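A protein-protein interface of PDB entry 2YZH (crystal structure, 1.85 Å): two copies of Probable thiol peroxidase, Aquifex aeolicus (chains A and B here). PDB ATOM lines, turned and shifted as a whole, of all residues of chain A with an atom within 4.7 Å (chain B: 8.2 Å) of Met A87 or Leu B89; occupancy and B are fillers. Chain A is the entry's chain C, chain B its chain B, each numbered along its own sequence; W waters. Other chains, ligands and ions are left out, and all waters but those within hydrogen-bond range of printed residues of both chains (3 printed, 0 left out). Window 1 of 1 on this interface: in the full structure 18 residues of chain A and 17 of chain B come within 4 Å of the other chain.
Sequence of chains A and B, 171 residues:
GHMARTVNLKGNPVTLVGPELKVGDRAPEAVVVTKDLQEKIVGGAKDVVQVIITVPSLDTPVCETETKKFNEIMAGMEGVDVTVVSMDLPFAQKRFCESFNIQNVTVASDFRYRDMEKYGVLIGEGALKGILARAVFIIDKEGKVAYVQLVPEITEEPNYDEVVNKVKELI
No residue of chain B comes within 4 Å of Ser A86. Met A87 touches just one residue of chain B: Leu B89 (3.4 Å). Of the printed residues of chain B, Asp A88 touches Leu B89 (3.3 Å). Of chain A, only Met A87 (3.4 Å), Asp A88 (3.3 Å) and Ile A131 (3.5 Å) come within 4 Å of Leu B89. Lys B94 touches none of the printed residues of chain A. Of the printed residues of chain A, Phe B111 touches Ile A131 (3.6 Å). The nearest residue of chain A that does not touch Leu B89 is Pro A56 (4.1 Å). The nearest printed residue of chain A that does not touch Asp B88 is Met A87 (6.2 Å).
Of the 14 printed residues of chain A, 5 touch a printed residue of chain B. Printed residues of chain A that touch a printed residue of chain B: Ser A57, Met A87, Asp A88, Leu A89 and Ile A131. Of the 24 printed residues of chain B, 5 touch a printed residue of chain A. Hydrophobic or aromatic side chains of chain B within 4 Å of the printed part of chain A: Met B87, Leu B89, Phe B91 and Phe B111. Among the printed residues, 7 pairs touch across the chains.
Ser A57 touches Phe B91. Met A87 touches Leu B89. Asp A88 touches Leu B89 (OD1 to CD1, 3.3 Å). Leu A89 touches Met B87. CD1 of Leu A89 touches OD1 of Asp B88, at 3.5 Å. Ile A131 touches Leu B89 (CD1 to CD2, 3.5 Å). Ile A131 touches Phe B111 (CD1 to CE1, 3.6 Å).
The side-chain hydroxyl (OG) of Ser A109 lies within hydrogen-bond range of the backbone carbonyl oxygen (O) of Asp A88 (2.5 Å). The backbone carbonyl oxygen (O) of Asp B88 sits at hydrogen-bond distance from the side-chain hydroxyl (OG) of Ser B109, 2.5 Å away. OG of Ser B109 sits close to N of Phe B111 (3.2 Å). The side-chain hydroxyl of Ser B86 lies within hydrogen-bond range of the side-chain carboxylate of Asp B88, at 2.6 Å. N of Leu B58 sits at hydrogen-bond distance from OD2 of Asp B88 (2.8 Å). The side-chain hydroxyl (OG) of Ser A86 sits at hydrogen-bond distance from the side-chain carboxylate (OD2) of Asp A88 (2.6 Å).
Water W3 bridges O of Arg B112 and NH1 of Arg A114. Water W1 bridges O of Met A87 (2.8 Å) and O of Met B87 (2.9 Å). Water W2 bridges N of Leu A89 (3.0 Å) and N of Leu B89 (3.0 Å).
Met A87 touches Leu B89, and with the chains exchanged Leu A89 touches Met B87. Asp A88 touches Leu B89, and with the chains exchanged Leu A89 touches Asp B88. 8 positions are printed for both chains. Of the 7 pairs that touch across the chains among the printed residues, 4 have their exchanged pair printed and touching as well.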
ATOM      1  N   VAL A  55      18.698  13.260 -24.937  1.00  0.00           N
ATOM      2  CA  VAL A  55      17.934  14.356 -24.352  1.00  0.00           C
ATOM      3  C   VAL A  55      18.059  14.284 -22.839  1.00  0.00           C
ATOM      4  O   VAL A  55      18.278  13.211 -22.282  1.00  0.00           O
ATOM      5  CB  VAL A  55      16.427  14.283 -24.722  1.00  0.00           C
ATOM      6  CG1 VAL A  55      16.246  14.430 -26.235  1.00  0.00           C
ATOM      7  CG2 VAL A  55      15.819  12.968 -24.228  1.00  0.00           C
ATOM      8  N   PRO A  56      17.937  15.430 -22.157  1.00  0.00           N
ATOM      9  CA  PRO A  56      18.035  15.471 -20.692  1.00  0.00           C
ATOM     10  C   PRO A  56      16.944  14.634 -20.020  1.00  0.00           C
ATOM     11  O   PRO A  56      17.219  13.822 -19.133  1.00  0.00           O
ATOM     12  CB  PRO A  56      17.895  16.959 -20.384  1.00  0.00           C
ATOM     13  CG  PRO A  56      18.526  17.600 -21.576  1.00  0.00           C
ATOM     14  CD  PRO A  56      17.956  16.793 -22.717  1.00  0.00           C
ATOM     15  N   SER A  57      15.701  14.831 -20.438  1.00  0.00           N
ATOM     16  CA  SER A  57      14.607  14.074 -19.857  1.00  0.00           C
ATOM     17  C   SER A  57      13.308  14.211 -20.619  1.00  0.00           C
ATOM     18  O   SER A  57      12.884  15.318 -20.952  1.00  0.00           O
ATOM     19  CB  SER A  57      14.377  14.495 -18.408  1.00  0.00           C
ATOM     20  OG  SER A  57      13.231  13.843 -17.881  1.00  0.00           O
ATOM     21  N   SER A  86      18.007   8.735 -22.831  1.00  0.00           N
ATOM     22  CA  SER A  86      18.080   9.679 -21.717  1.00  0.00           C
ATOM     23  C   SER A  86      18.357   8.898 -20.440  1.00  0.00           C
ATOM     24  O   SER A  86      18.435   7.663 -20.459  1.00  0.00           O
ATOM     25  CB  SER A  86      16.762  10.445 -21.555  1.00  0.00           C
ATOM     26  OG  SER A  86      15.749   9.614 -21.007  1.00  0.00           O
ATOM     27  N   MET A  87      18.510   9.614 -19.331  1.00  0.00           N
ATOM     28  CA  MET A  87      18.750   8.958 -18.049  1.00  0.00           C
ATOM     29  C   MET A  87      17.435   8.674 -17.321  1.00  0.00           C
ATOM     30  O   MET A  87      17.442   8.231 -16.165  1.00  0.00           O
ATOM     31  CB  MET A  87      19.670   9.809 -17.170  1.00  0.00           C
ATOM     32  CG  MET A  87      21.074  10.004 -17.733  1.00  0.00           C
ATOM     33  SD  MET A  87      21.952   8.445 -18.003  1.00  0.00           S
ATOM     34  CE  MET A  87      22.152   7.919 -16.339  1.00  0.00           C
ATOM     35  N   ASP A  88      16.305   8.927 -17.988  1.00  0.00           N
ATOM     36  CA  ASP A  88      15.000   8.640 -17.377  1.00  0.00           C
ATOM     37  C   ASP A  88      14.955   7.125 -17.178  1.00  0.00           C
ATOM     38  O   ASP A  88      15.519   6.387 -17.984  1.00  0.00           O
ATOM     39  CB  ASP A  88      13.831   8.994 -18.311  1.00  0.00           C
ATOM     40  CG  ASP A  88      13.735  10.471 -18.626  1.00  0.00           C
ATOM     41  OD1 ASP A  88      13.592  11.282 -17.692  1.00  0.00           O
ATOM     42  OD2 ASP A  88      13.786  10.822 -19.827  1.00  0.00           O
ATOM     43  N   LEU A  89      14.301   6.652 -16.121  1.00  0.00           N
ATOM     44  CA  LEU A  89      14.189   5.212 -15.940  1.00  0.00           C
ATOM     45  C   LEU A  89      13.210   4.687 -16.987  1.00  0.00           C
ATOM     46  O   LEU A  89      12.384   5.438 -17.512  1.00  0.00           O
ATOM     47  CB  LEU A  89      13.658   4.858 -14.548  1.00  0.00           C
ATOM     48  CG  LEU A  89      14.607   5.081 -13.370  1.00  0.00           C
ATOM     49  CD1 LEU A  89      13.982   4.487 -12.105  1.00  0.00           C
ATOM     50  CD2 LEU A  89      15.956   4.419 -13.659  1.00  0.00           C
ATOM     51  N   SER A 109      16.754   3.868 -21.979  1.00  0.00           N
ATOM     52  CA  SER A 109      17.376   4.495 -20.823  1.00  0.00           C
ATOM     53  C   SER A 109      18.831   4.076 -20.666  1.00  0.00           C
ATOM     54  O   SER A 109      19.163   2.903 -20.836  1.00  0.00           O
ATOM     55  CB  SER A 109      16.605   4.107 -19.558  1.00  0.00           C
ATOM     56  OG  SER A 109      17.242   4.618 -18.403  1.00  0.00           O
ATOM     57  N   ASP A 110      19.691   5.034 -20.323  1.00  0.00           N
ATOM     58  CA  ASP A 110      21.108   4.753 -20.127  1.00  0.00           C
ATOM     59  C   ASP A 110      21.441   4.749 -18.630  1.00  0.00           C
ATOM     60  O   ASP A 110      22.593   4.911 -18.241  1.00  0.00           O
ATOM     61  CB  ASP A 110      21.941   5.810 -20.859  1.00  0.00           C
ATOM     62  CG  ASP A 110      23.427   5.518 -20.830  1.00  0.00           C
ATOM     63  OD1 ASP A 110      23.820   4.327 -20.831  1.00  0.00           O
ATOM     64  OD2 ASP A 110      24.207   6.492 -20.828  1.00  0.00           O
ATOM     65  N   PHE A 111      20.426   4.542 -17.796  1.00  0.00           N
ATOM     66  CA  PHE A 111      20.628   4.549 -16.349  1.00  0.00           C
ATOM     67  C   PHE A 111      21.536   3.443 -15.815  1.00  0.00           C
ATOM     68  O   PHE A 111      22.256   3.650 -14.840  1.00  0.00           O
ATOM     69  CB  PHE A 111      19.275   4.458 -15.622  1.00  0.00           C
ATOM     70  CG  PHE A 111      18.799   3.037 -15.388  1.00  0.00           C
ATOM     71  CD1 PHE A 111      19.145   2.354 -14.221  1.00  0.00           C
ATOM     72  CD2 PHE A 111      18.046   2.373 -16.351  1.00  0.00           C
ATOM     73  CE1 PHE A 111      18.755   1.032 -14.016  1.00  0.00           C
ATOM     74  CE2 PHE A 111      17.647   1.044 -16.157  1.00  0.00           C
ATOM     75  CZ  PHE A 111      18.005   0.374 -14.986  1.00  0.00           C
ATOM     76  N   ARG A 114      25.368   3.961 -18.007  1.00  0.00           N
ATOM     77  CA  ARG A 114      25.714   5.336 -18.346  1.00  0.00           C
ATOM     78  C   ARG A 114      26.753   5.336 -19.466  1.00  0.00           C
ATOM     79  O   ARG A 114      27.750   6.061 -19.415  1.00  0.00           O
ATOM     80  CB  ARG A 114      26.252   6.087 -17.119  1.00  0.00           C
ATOM     81  CG  ARG A 114      26.116   7.604 -17.266  1.00  0.00           C
ATOM     82  CD  ARG A 114      26.308   8.348 -15.949  1.00  0.00           C
ATOM     83  NE  ARG A 114      27.695   8.328 -15.495  1.00  0.00           N
ATOM     84  CZ  ARG A 114      28.146   9.008 -14.444  1.00  0.00           C
ATOM     85  NH1 ARG A 114      27.319   9.763 -13.733  1.00  0.00           N
ATOM     86  NH2 ARG A 114      29.429   8.941 -14.111  1.00  0.00           N
ATOM     87  N   GLY A 130      25.163  14.837 -14.395  1.00  0.00           N
ATOM     88  CA  GLY A 130      24.752  13.439 -14.408  1.00  0.00           C
ATOM     89  C   GLY A 130      23.681  13.102 -15.429  1.00  0.00           C
ATOM     90  O   GLY A 130      23.331  11.934 -15.596  1.00  0.00           O
ATOM     91  N   ILE A 131      23.158  14.132 -16.100  1.00  0.00           N
ATOM     92  CA  ILE A 131      22.125  13.994 -17.128  1.00  0.00           C
ATOM     93  C   ILE A 131      22.791  14.190 -18.497  1.00  0.00           C
ATOM     94  O   ILE A 131      23.900  14.714 -18.573  1.00  0.00           O
ATOM     95  CB  ILE A 131      21.023  15.076 -16.930  1.00  0.00           C
ATOM     96  CG1 ILE A 131      20.359  14.892 -15.561  1.00  0.00           C
ATOM     97  CG2 ILE A 131      20.004  15.013 -18.045  1.00  0.00           C
ATOM     98  CD1 ILE A 131      19.727  13.538 -15.363  1.00  0.00           C
ATOM     99  N   LEU A 132      22.129  13.770 -19.573  1.00  0.00           N
ATOM    100  CA  LEU A 132      22.710  13.913 -20.908  1.00  0.00           C
ATOM    101  C   LEU A 132      22.313  15.229 -21.579  1.00  0.00           C
ATOM    102  O   LEU A 132      21.180  15.679 -21.439  1.00  0.00           O
ATOM    103  CB  LEU A 132      22.271  12.754 -21.811  1.00  0.00           C
ATOM    104  CG  LEU A 132      22.411  11.318 -21.290  1.00  0.00           C
ATOM    105  CD1 LEU A 132      22.030  10.337 -22.397  1.00  0.00           C
ATOM    106  CD2 LEU A 132      23.837  11.070 -20.830  1.00  0.00           C
ATOM    107  N   VAL B  33      18.922  13.956  -4.571  1.00  0.00           N
ATOM    108  CA  VAL B  33      18.412  15.157  -5.236  1.00  0.00           C
ATOM    109  C   VAL B  33      16.889  15.267  -5.158  1.00  0.00           C
ATOM    110  O   VAL B  33      16.174  14.348  -5.563  1.00  0.00           O
ATOM    111  CB  VAL B  33      18.839  15.148  -6.731  1.00  0.00           C
ATOM    112  CG1 VAL B  33      18.401  16.437  -7.424  1.00  0.00           C
ATOM    113  CG2 VAL B  33      20.342  14.962  -6.838  1.00  0.00           C
ATOM    114  N   THR B  34      16.387  16.396  -4.654  1.00  0.00           N
ATOM    115  CA  THR B  34      14.943  16.587  -4.534  1.00  0.00           C
ATOM    116  C   THR B  34      14.318  17.084  -5.841  1.00  0.00           C
ATOM    117  O   THR B  34      15.028  17.390  -6.796  1.00  0.00           O
ATOM    118  CB  THR B  34      14.605  17.550  -3.371  1.00  0.00           C
ATOM    119  OG1 THR B  34      15.298  18.786  -3.545  1.00  0.00           O
ATOM    120  CG2 THR B  34      15.026  16.934  -2.042  1.00  0.00           C
ATOM    121  N   LYS B  35      12.991  17.160  -5.883  1.00  0.00           N
ATOM    122  CA  LYS B  35      12.293  17.577  -7.098  1.00  0.00           C
ATOM    123  C   LYS B  35      12.657  18.955  -7.637  1.00  0.00           C
ATOM    124  O   LYS B  35      12.423  19.239  -8.810  1.00  0.00           O
ATOM    125  CB  LYS B  35      10.776  17.485  -6.895  1.00  0.00           C
ATOM    126  CG  LYS B  35      10.245  18.296  -5.732  1.00  0.00           C
ATOM    127  CD  LYS B  35       8.785  17.968  -5.472  1.00  0.00           C
ATOM    128  CE  LYS B  35       8.268  18.717  -4.255  1.00  0.00           C
ATOM    129  NZ  LYS B  35       6.869  18.333  -3.939  1.00  0.00           N
ATOM    130  N   LEU B  37      15.679  19.976  -7.767  1.00  0.00           N
ATOM    131  CA  LEU B  37      17.075  19.805  -8.154  1.00  0.00           C
ATOM    132  C   LEU B  37      18.090  20.241  -7.105  1.00  0.00           C
ATOM    133  O   LEU B  37      19.262  20.443  -7.415  1.00  0.00           O
ATOM    134  CB  LEU B  37      17.346  20.519  -9.479  1.00  0.00           C
ATOM    135  CG  LEU B  37      16.400  20.095 -10.608  1.00  0.00           C
ATOM    136  CD1 LEU B  37      16.753  20.851 -11.871  1.00  0.00           C
ATOM    137  CD2 LEU B  37      16.495  18.596 -10.837  1.00  0.00           C
ATOM    138  N   SER B  57      10.577   2.329  -8.188  1.00  0.00           N
ATOM    139  CA  SER B  57      10.165   3.462  -9.019  1.00  0.00           C
ATOM    140  C   SER B  57       8.775   4.001  -8.701  1.00  0.00           C
ATOM    141  O   SER B  57       7.817   3.237  -8.600  1.00  0.00           O
ATOM    142  CB  SER B  57      10.208   3.079 -10.498  1.00  0.00           C
ATOM    143  OG  SER B  57       9.744   4.151 -11.310  1.00  0.00           O
ATOM    144  N   LEU B  58       8.667   5.322  -8.565  1.00  0.00           N
ATOM    145  CA  LEU B  58       7.384   5.957  -8.279  1.00  0.00           C
ATOM    146  C   LEU B  58       6.451   5.850  -9.482  1.00  0.00           C
ATOM    147  O   LEU B  58       5.256   6.145  -9.380  1.00  0.00           O
ATOM    148  CB  LEU B  58       7.587   7.428  -7.914  1.00  0.00           C
ATOM    149  CG  LEU B  58       8.351   7.681  -6.613  1.00  0.00           C
ATOM    150  CD1 LEU B  58       8.541   9.175  -6.408  1.00  0.00           C
ATOM    151  CD2 LEU B  58       7.582   7.075  -5.451  1.00  0.00           C
ATOM    152  N   ASP B  59       7.003   5.441 -10.620  1.00  0.00           N
ATOM    153  CA  ASP B  59       6.209   5.279 -11.828  1.00  0.00           C
ATOM    154  C   ASP B  59       5.653   3.864 -11.934  1.00  0.00           C
ATOM    155  O   ASP B  59       5.238   3.440 -13.012  1.00  0.00           O
ATOM    156  CB  ASP B  59       7.030   5.599 -13.084  1.00  0.00           C
ATOM    157  CG  ASP B  59       7.067   7.082 -13.391  1.00  0.00           C
ATOM    158  OD1 ASP B  59       6.036   7.749 -13.182  1.00  0.00           O
ATOM    159  OD2 ASP B  59       8.113   7.581 -13.854  1.00  0.00           O
ATOM    160  N   SER B  86      14.461   6.796  -4.653  1.00  0.00           N
ATOM    161  CA  SER B  86      14.434   5.855  -5.771  1.00  0.00           C
ATOM    162  C   SER B  86      15.439   6.297  -6.823  1.00  0.00           C
ATOM    163  O   SER B  86      16.098   7.327  -6.672  1.00  0.00           O
ATOM    164  CB  SER B  86      13.052   5.814  -6.416  1.00  0.00           C
ATOM    165  OG  SER B  86      12.831   6.986  -7.192  1.00  0.00           O
ATOM    166  N   MET B  87      15.558   5.518  -7.892  1.00  0.00           N
ATOM    167  CA  MET B  87      16.471   5.881  -8.963  1.00  0.00           C
ATOM    168  C   MET B  87      15.761   6.723 -10.022  1.00  0.00           C
ATOM    169  O   MET B  87      16.360   7.073 -11.032  1.00  0.00           O
ATOM    170  CB  MET B  87      17.083   4.639  -9.613  1.00  0.00           C
ATOM    171  CG  MET B  87      18.055   3.876  -8.713  1.00  0.00           C
ATOM    172  SD  MET B  87      19.383   4.907  -8.019  1.00  0.00           S
ATOM    173  CE  MET B  87      20.491   5.042  -9.393  1.00  0.00           C
ATOM    174  N   ASP B  88      14.487   7.036  -9.800  1.00  0.00           N
ATOM    175  CA  ASP B  88      13.745   7.871 -10.747  1.00  0.00           C
ATOM    176  C   ASP B  88      14.467   9.201 -10.831  1.00  0.00           C
ATOM    177  O   ASP B  88      15.039   9.652  -9.842  1.00  0.00           O
ATOM    178  CB  ASP B  88      12.331   8.185 -10.248  1.00  0.00           C
ATOM    179  CG  ASP B  88      11.461   6.968 -10.118  1.00  0.00           C
ATOM    180  OD1 ASP B  88      11.202   6.310 -11.140  1.00  0.00           O
ATOM    181  OD2 ASP B  88      11.025   6.679  -8.984  1.00  0.00           O
ATOM    182  N   LEU B  89      14.438   9.839 -11.997  1.00  0.00           N
ATOM    183  CA  LEU B  89      15.062  11.148 -12.116  1.00  0.00           C
ATOM    184  C   LEU B  89      14.144  12.129 -11.386  1.00  0.00           C
ATOM    185  O   LEU B  89      12.947  11.880 -11.248  1.00  0.00           O
ATOM    186  CB  LEU B  89      15.185  11.581 -13.580  1.00  0.00           C
ATOM    187  CG  LEU B  89      16.305  10.988 -14.434  1.00  0.00           C
ATOM    188  CD1 LEU B  89      16.303  11.697 -15.793  1.00  0.00           C
ATOM    189  CD2 LEU B  89      17.659  11.171 -13.743  1.00  0.00           C
ATOM    190  N   PRO B  90      14.699  13.246 -10.898  1.00  0.00           N
ATOM    191  CA  PRO B  90      13.911  14.256 -10.186  1.00  0.00           C
ATOM    192  C   PRO B  90      12.671  14.705 -10.979  1.00  0.00           C
ATOM    193  O   PRO B  90      11.637  15.041 -10.399  1.00  0.00           O
ATOM    194  CB  PRO B  90      14.915  15.389  -9.988  1.00  0.00           C
ATOM    195  CG  PRO B  90      16.209  14.648  -9.814  1.00  0.00           C
ATOM    196  CD  PRO B  90      16.124  13.615 -10.923  1.00  0.00           C
ATOM    197  N   PHE B  91      12.773  14.700 -12.303  1.00  0.00           N
ATOM    198  CA  PHE B  91      11.660  15.130 -13.151  1.00  0.00           C
ATOM    199  C   PHE B  91      10.439  14.229 -13.030  1.00  0.00           C
ATOM    200  O   PHE B  91       9.303  14.709 -13.042  1.00  0.00           O
ATOM    201  CB  PHE B  91      12.134  15.218 -14.601  1.00  0.00           C
ATOM    202  CG  PHE B  91      13.404  15.998 -14.756  1.00  0.00           C
ATOM    203  CD1 PHE B  91      13.448  17.349 -14.428  1.00  0.00           C
ATOM    204  CD2 PHE B  91      14.573  15.372 -15.176  1.00  0.00           C
ATOM    205  CE1 PHE B  91      14.644  18.066 -14.515  1.00  0.00           C
ATOM    206  CE2 PHE B  91      15.771  16.081 -15.266  1.00  0.00           C
ATOM    207  CZ  PHE B  91      15.807  17.428 -14.935  1.00  0.00           C
ATOM    208  N   ALA B  92      10.667  12.926 -12.905  1.00  0.00           N
ATOM    209  CA  ALA B  92       9.564  11.990 -12.748  1.00  0.00           C
ATOM    210  C   ALA B  92       8.980  12.181 -11.357  1.00  0.00           C
ATOM    211  O   ALA B  92       7.762  12.138 -11.171  1.00  0.00           O
ATOM    212  CB  ALA B  92      10.054  10.553 -12.916  1.00  0.00           C
ATOM    213  N   GLN B  93       9.853  12.401 -10.379  1.00  0.00           N
ATOM    214  CA  GLN B  93       9.403  12.587  -9.006  1.00  0.00           C
ATOM    215  C   GLN B  93       8.610  13.879  -8.867  1.00  0.00           C
ATOM    216  O   GLN B  93       7.642  13.943  -8.110  1.00  0.00           O
ATOM    217  CB  GLN B  93      10.594  12.593  -8.042  1.00  0.00           C
ATOM    218  CG  GLN B  93      11.423  11.299  -8.064  1.00  0.00           C
ATOM    219  CD  GLN B  93      12.228  11.108  -6.792  1.00  0.00           C
ATOM    220  OE1 GLN B  93      12.683  12.077  -6.188  1.00  0.00           O
ATOM    221  NE2 GLN B  93      12.415   9.854  -6.384  1.00  0.00           N
ATOM    222  N   LYS B  94       9.021  14.912  -9.591  1.00  0.00           N
ATOM    223  CA  LYS B  94       8.302  16.177  -9.535  1.00  0.00           C
ATOM    224  C   LYS B  94       6.889  15.943 -10.063  1.00  0.00           C
ATOM    225  O   LYS B  94       5.908  16.398  -9.467  1.00  0.00           O
ATOM    226  CB  LYS B  94       9.011  17.240 -10.380  1.00  0.00           C
ATOM    227  CG  LYS B  94       8.336  18.600 -10.339  1.00  0.00           C
ATOM    228  CD  LYS B  94       9.185  19.660 -11.019  1.00  0.00           C
ATOM    229  CE  LYS B  94       8.502  21.020 -10.974  1.00  0.00           C
ATOM    230  NZ  LYS B  94       8.162  21.440  -9.582  1.00  0.00           N
ATOM    231  N   ARG B  95       6.791  15.218 -11.175  1.00  0.00           N
ATOM    232  CA  ARG B  95       5.498  14.911 -11.784  1.00  0.00           C
ATOM    233  C   ARG B  95       4.614  14.122 -10.826  1.00  0.00           C
ATOM    234  O   ARG B  95       3.404  14.345 -10.761  1.00  0.00           O
ATOM    235  CB  ARG B  95       5.692  14.116 -13.079  1.00  0.00           C
ATOM    236  CG  ARG B  95       4.389  13.674 -13.730  1.00  0.00           C
ATOM    237  CD  ARG B  95       4.620  13.093 -15.117  1.00  0.00           C
ATOM    238  NE  ARG B  95       5.610  12.020 -15.100  1.00  0.00           N
ATOM    239  CZ  ARG B  95       5.917  11.262 -16.147  1.00  0.00           C
ATOM    240  NH1 ARG B  95       5.311  11.454 -17.311  1.00  0.00           N
ATOM    241  NH2 ARG B  95       6.830  10.305 -16.025  1.00  0.00           N
ATOM    242  N   PHE B  96       5.224  13.199 -10.087  1.00  0.00           N
ATOM    243  CA  PHE B  96       4.495  12.378  -9.128  1.00  0.00           C
ATOM    244  C   PHE B  96       3.868  13.248  -8.043  1.00  0.00           C
ATOM    245  O   PHE B  96       2.703  13.064  -7.685  1.00  0.00           O
ATOM    246  CB  PHE B  96       5.438  11.364  -8.472  1.00  0.00           C
ATOM    247  CG  PHE B  96       4.759  10.456  -7.478  1.00  0.00           C
ATOM    248  CD1 PHE B  96       4.076   9.323  -7.903  1.00  0.00           C
ATOM    249  CD2 PHE B  96       4.802  10.739  -6.118  1.00  0.00           C
ATOM    250  CE1 PHE B  96       3.448   8.479  -6.987  1.00  0.00           C
ATOM    251  CE2 PHE B  96       4.176   9.903  -5.191  1.00  0.00           C
ATOM    252  CZ  PHE B  96       3.499   8.772  -5.628  1.00  0.00           C
ATOM    253  N   VAL B 107      10.318  13.240  -1.354  1.00  0.00           N
ATOM    254  CA  VAL B 107      10.762  12.256  -2.332  1.00  0.00           C
ATOM    255  C   VAL B 107      12.121  12.728  -2.838  1.00  0.00           C
ATOM    256  O   VAL B 107      12.345  13.927  -3.003  1.00  0.00           O
ATOM    257  CB  VAL B 107       9.772  12.124  -3.521  1.00  0.00           C
ATOM    258  CG1 VAL B 107       8.419  11.648  -3.018  1.00  0.00           C
ATOM    259  CG2 VAL B 107       9.633  13.450  -4.242  1.00  0.00           C
ATOM    260  N   ALA B 108      13.040  11.796  -3.063  1.00  0.00           N
ATOM    261  CA  ALA B 108      14.366  12.169  -3.539  1.00  0.00           C
ATOM    262  C   ALA B 108      14.923  11.130  -4.496  1.00  0.00           C
ATOM    263  O   ALA B 108      14.565   9.959  -4.424  1.00  0.00           O
ATOM    264  CB  ALA B 108      15.318  12.356  -2.360  1.00  0.00           C
ATOM    265  N   SER B 109      15.804  11.579  -5.385  1.00  0.00           N
ATOM    266  CA  SER B 109      16.428  10.710  -6.371  1.00  0.00           C
ATOM    267  C   SER B 109      17.884  10.428  -6.034  1.00  0.00           C
ATOM    268  O   SER B 109      18.629  11.324  -5.644  1.00  0.00           O
ATOM    269  CB  SER B 109      16.352  11.352  -7.760  1.00  0.00           C
ATOM    270  OG  SER B 109      17.073  10.579  -8.707  1.00  0.00           O
ATOM    271  N   ASP B 110      18.287   9.175  -6.212  1.00  0.00           N
ATOM    272  CA  ASP B 110      19.654   8.749  -5.942  1.00  0.00           C
ATOM    273  C   ASP B 110      20.399   8.498  -7.259  1.00  0.00           C
ATOM    274  O   ASP B 110      21.427   7.823  -7.289  1.00  0.00           O
ATOM    275  CB  ASP B 110      19.608   7.477  -5.095  1.00  0.00           C
ATOM    276  CG  ASP B 110      20.954   7.073  -4.565  1.00  0.00           C
ATOM    277  OD1 ASP B 110      21.768   7.961  -4.233  1.00  0.00           O
ATOM    278  OD2 ASP B 110      21.186   5.848  -4.459  1.00  0.00           O
ATOM    279  N   PHE B 111      19.890   9.068  -8.348  1.00  0.00           N
ATOM    280  CA  PHE B 111      20.503   8.868  -9.661  1.00  0.00           C
ATOM    281  C   PHE B 111      21.929   9.393  -9.784  1.00  0.00           C
ATOM    282  O   PHE B 111      22.761   8.799 -10.477  1.00  0.00           O
ATOM    283  CB  PHE B 111      19.642   9.531 -10.754  1.00  0.00           C
ATOM    284  CG  PHE B 111      19.998  10.980 -11.018  1.00  0.00           C
ATOM    285  CD1 PHE B 111      20.919  11.316 -12.009  1.00  0.00           C
ATOM    286  CD2 PHE B 111      19.442  11.996 -10.253  1.00  0.00           C
ATOM    287  CE1 PHE B 111      21.283  12.646 -12.229  1.00  0.00           C
ATOM    288  CE2 PHE B 111      19.800  13.332 -10.465  1.00  0.00           C
ATOM    289  CZ  PHE B 111      20.723  13.652 -11.456  1.00  0.00           C
ATOM    290  N   ARG B 112      22.213  10.507  -9.116  1.00  0.00           N
ATOM    291  CA  ARG B 112      23.523  11.140  -9.229  1.00  0.00           C
ATOM    292  C   ARG B 112      24.727  10.401  -8.655  1.00  0.00           C
ATOM    293  O   ARG B 112      25.755  10.287  -9.325  1.00  0.00           O
ATOM    294  CB  ARG B 112      23.459  12.559  -8.650  1.00  0.00           C
ATOM    295  CG  ARG B 112      24.764  13.349  -8.764  1.00  0.00           C
ATOM    296  CD  ARG B 112      24.515  14.832  -8.522  1.00  0.00           C
ATOM    297  NE  ARG B 112      23.836  15.445  -9.665  1.00  0.00           N
ATOM    298  CZ  ARG B 112      23.085  16.541  -9.599  1.00  0.00           C
ATOM    299  NH1 ARG B 112      22.903  17.158  -8.441  1.00  0.00           N
ATOM    300  NH2 ARG B 112      22.519  17.026 -10.699  1.00  0.00           N
HETATM  301  O   HOH W   1      17.707   7.437 -13.530  1.00  0.00           O
HETATM  302  O   HOH W   2      12.975   8.575 -14.290  1.00  0.00           O
HETATM  303  O   HOH W   3      25.852  11.358 -11.838  1.00  0.00           O
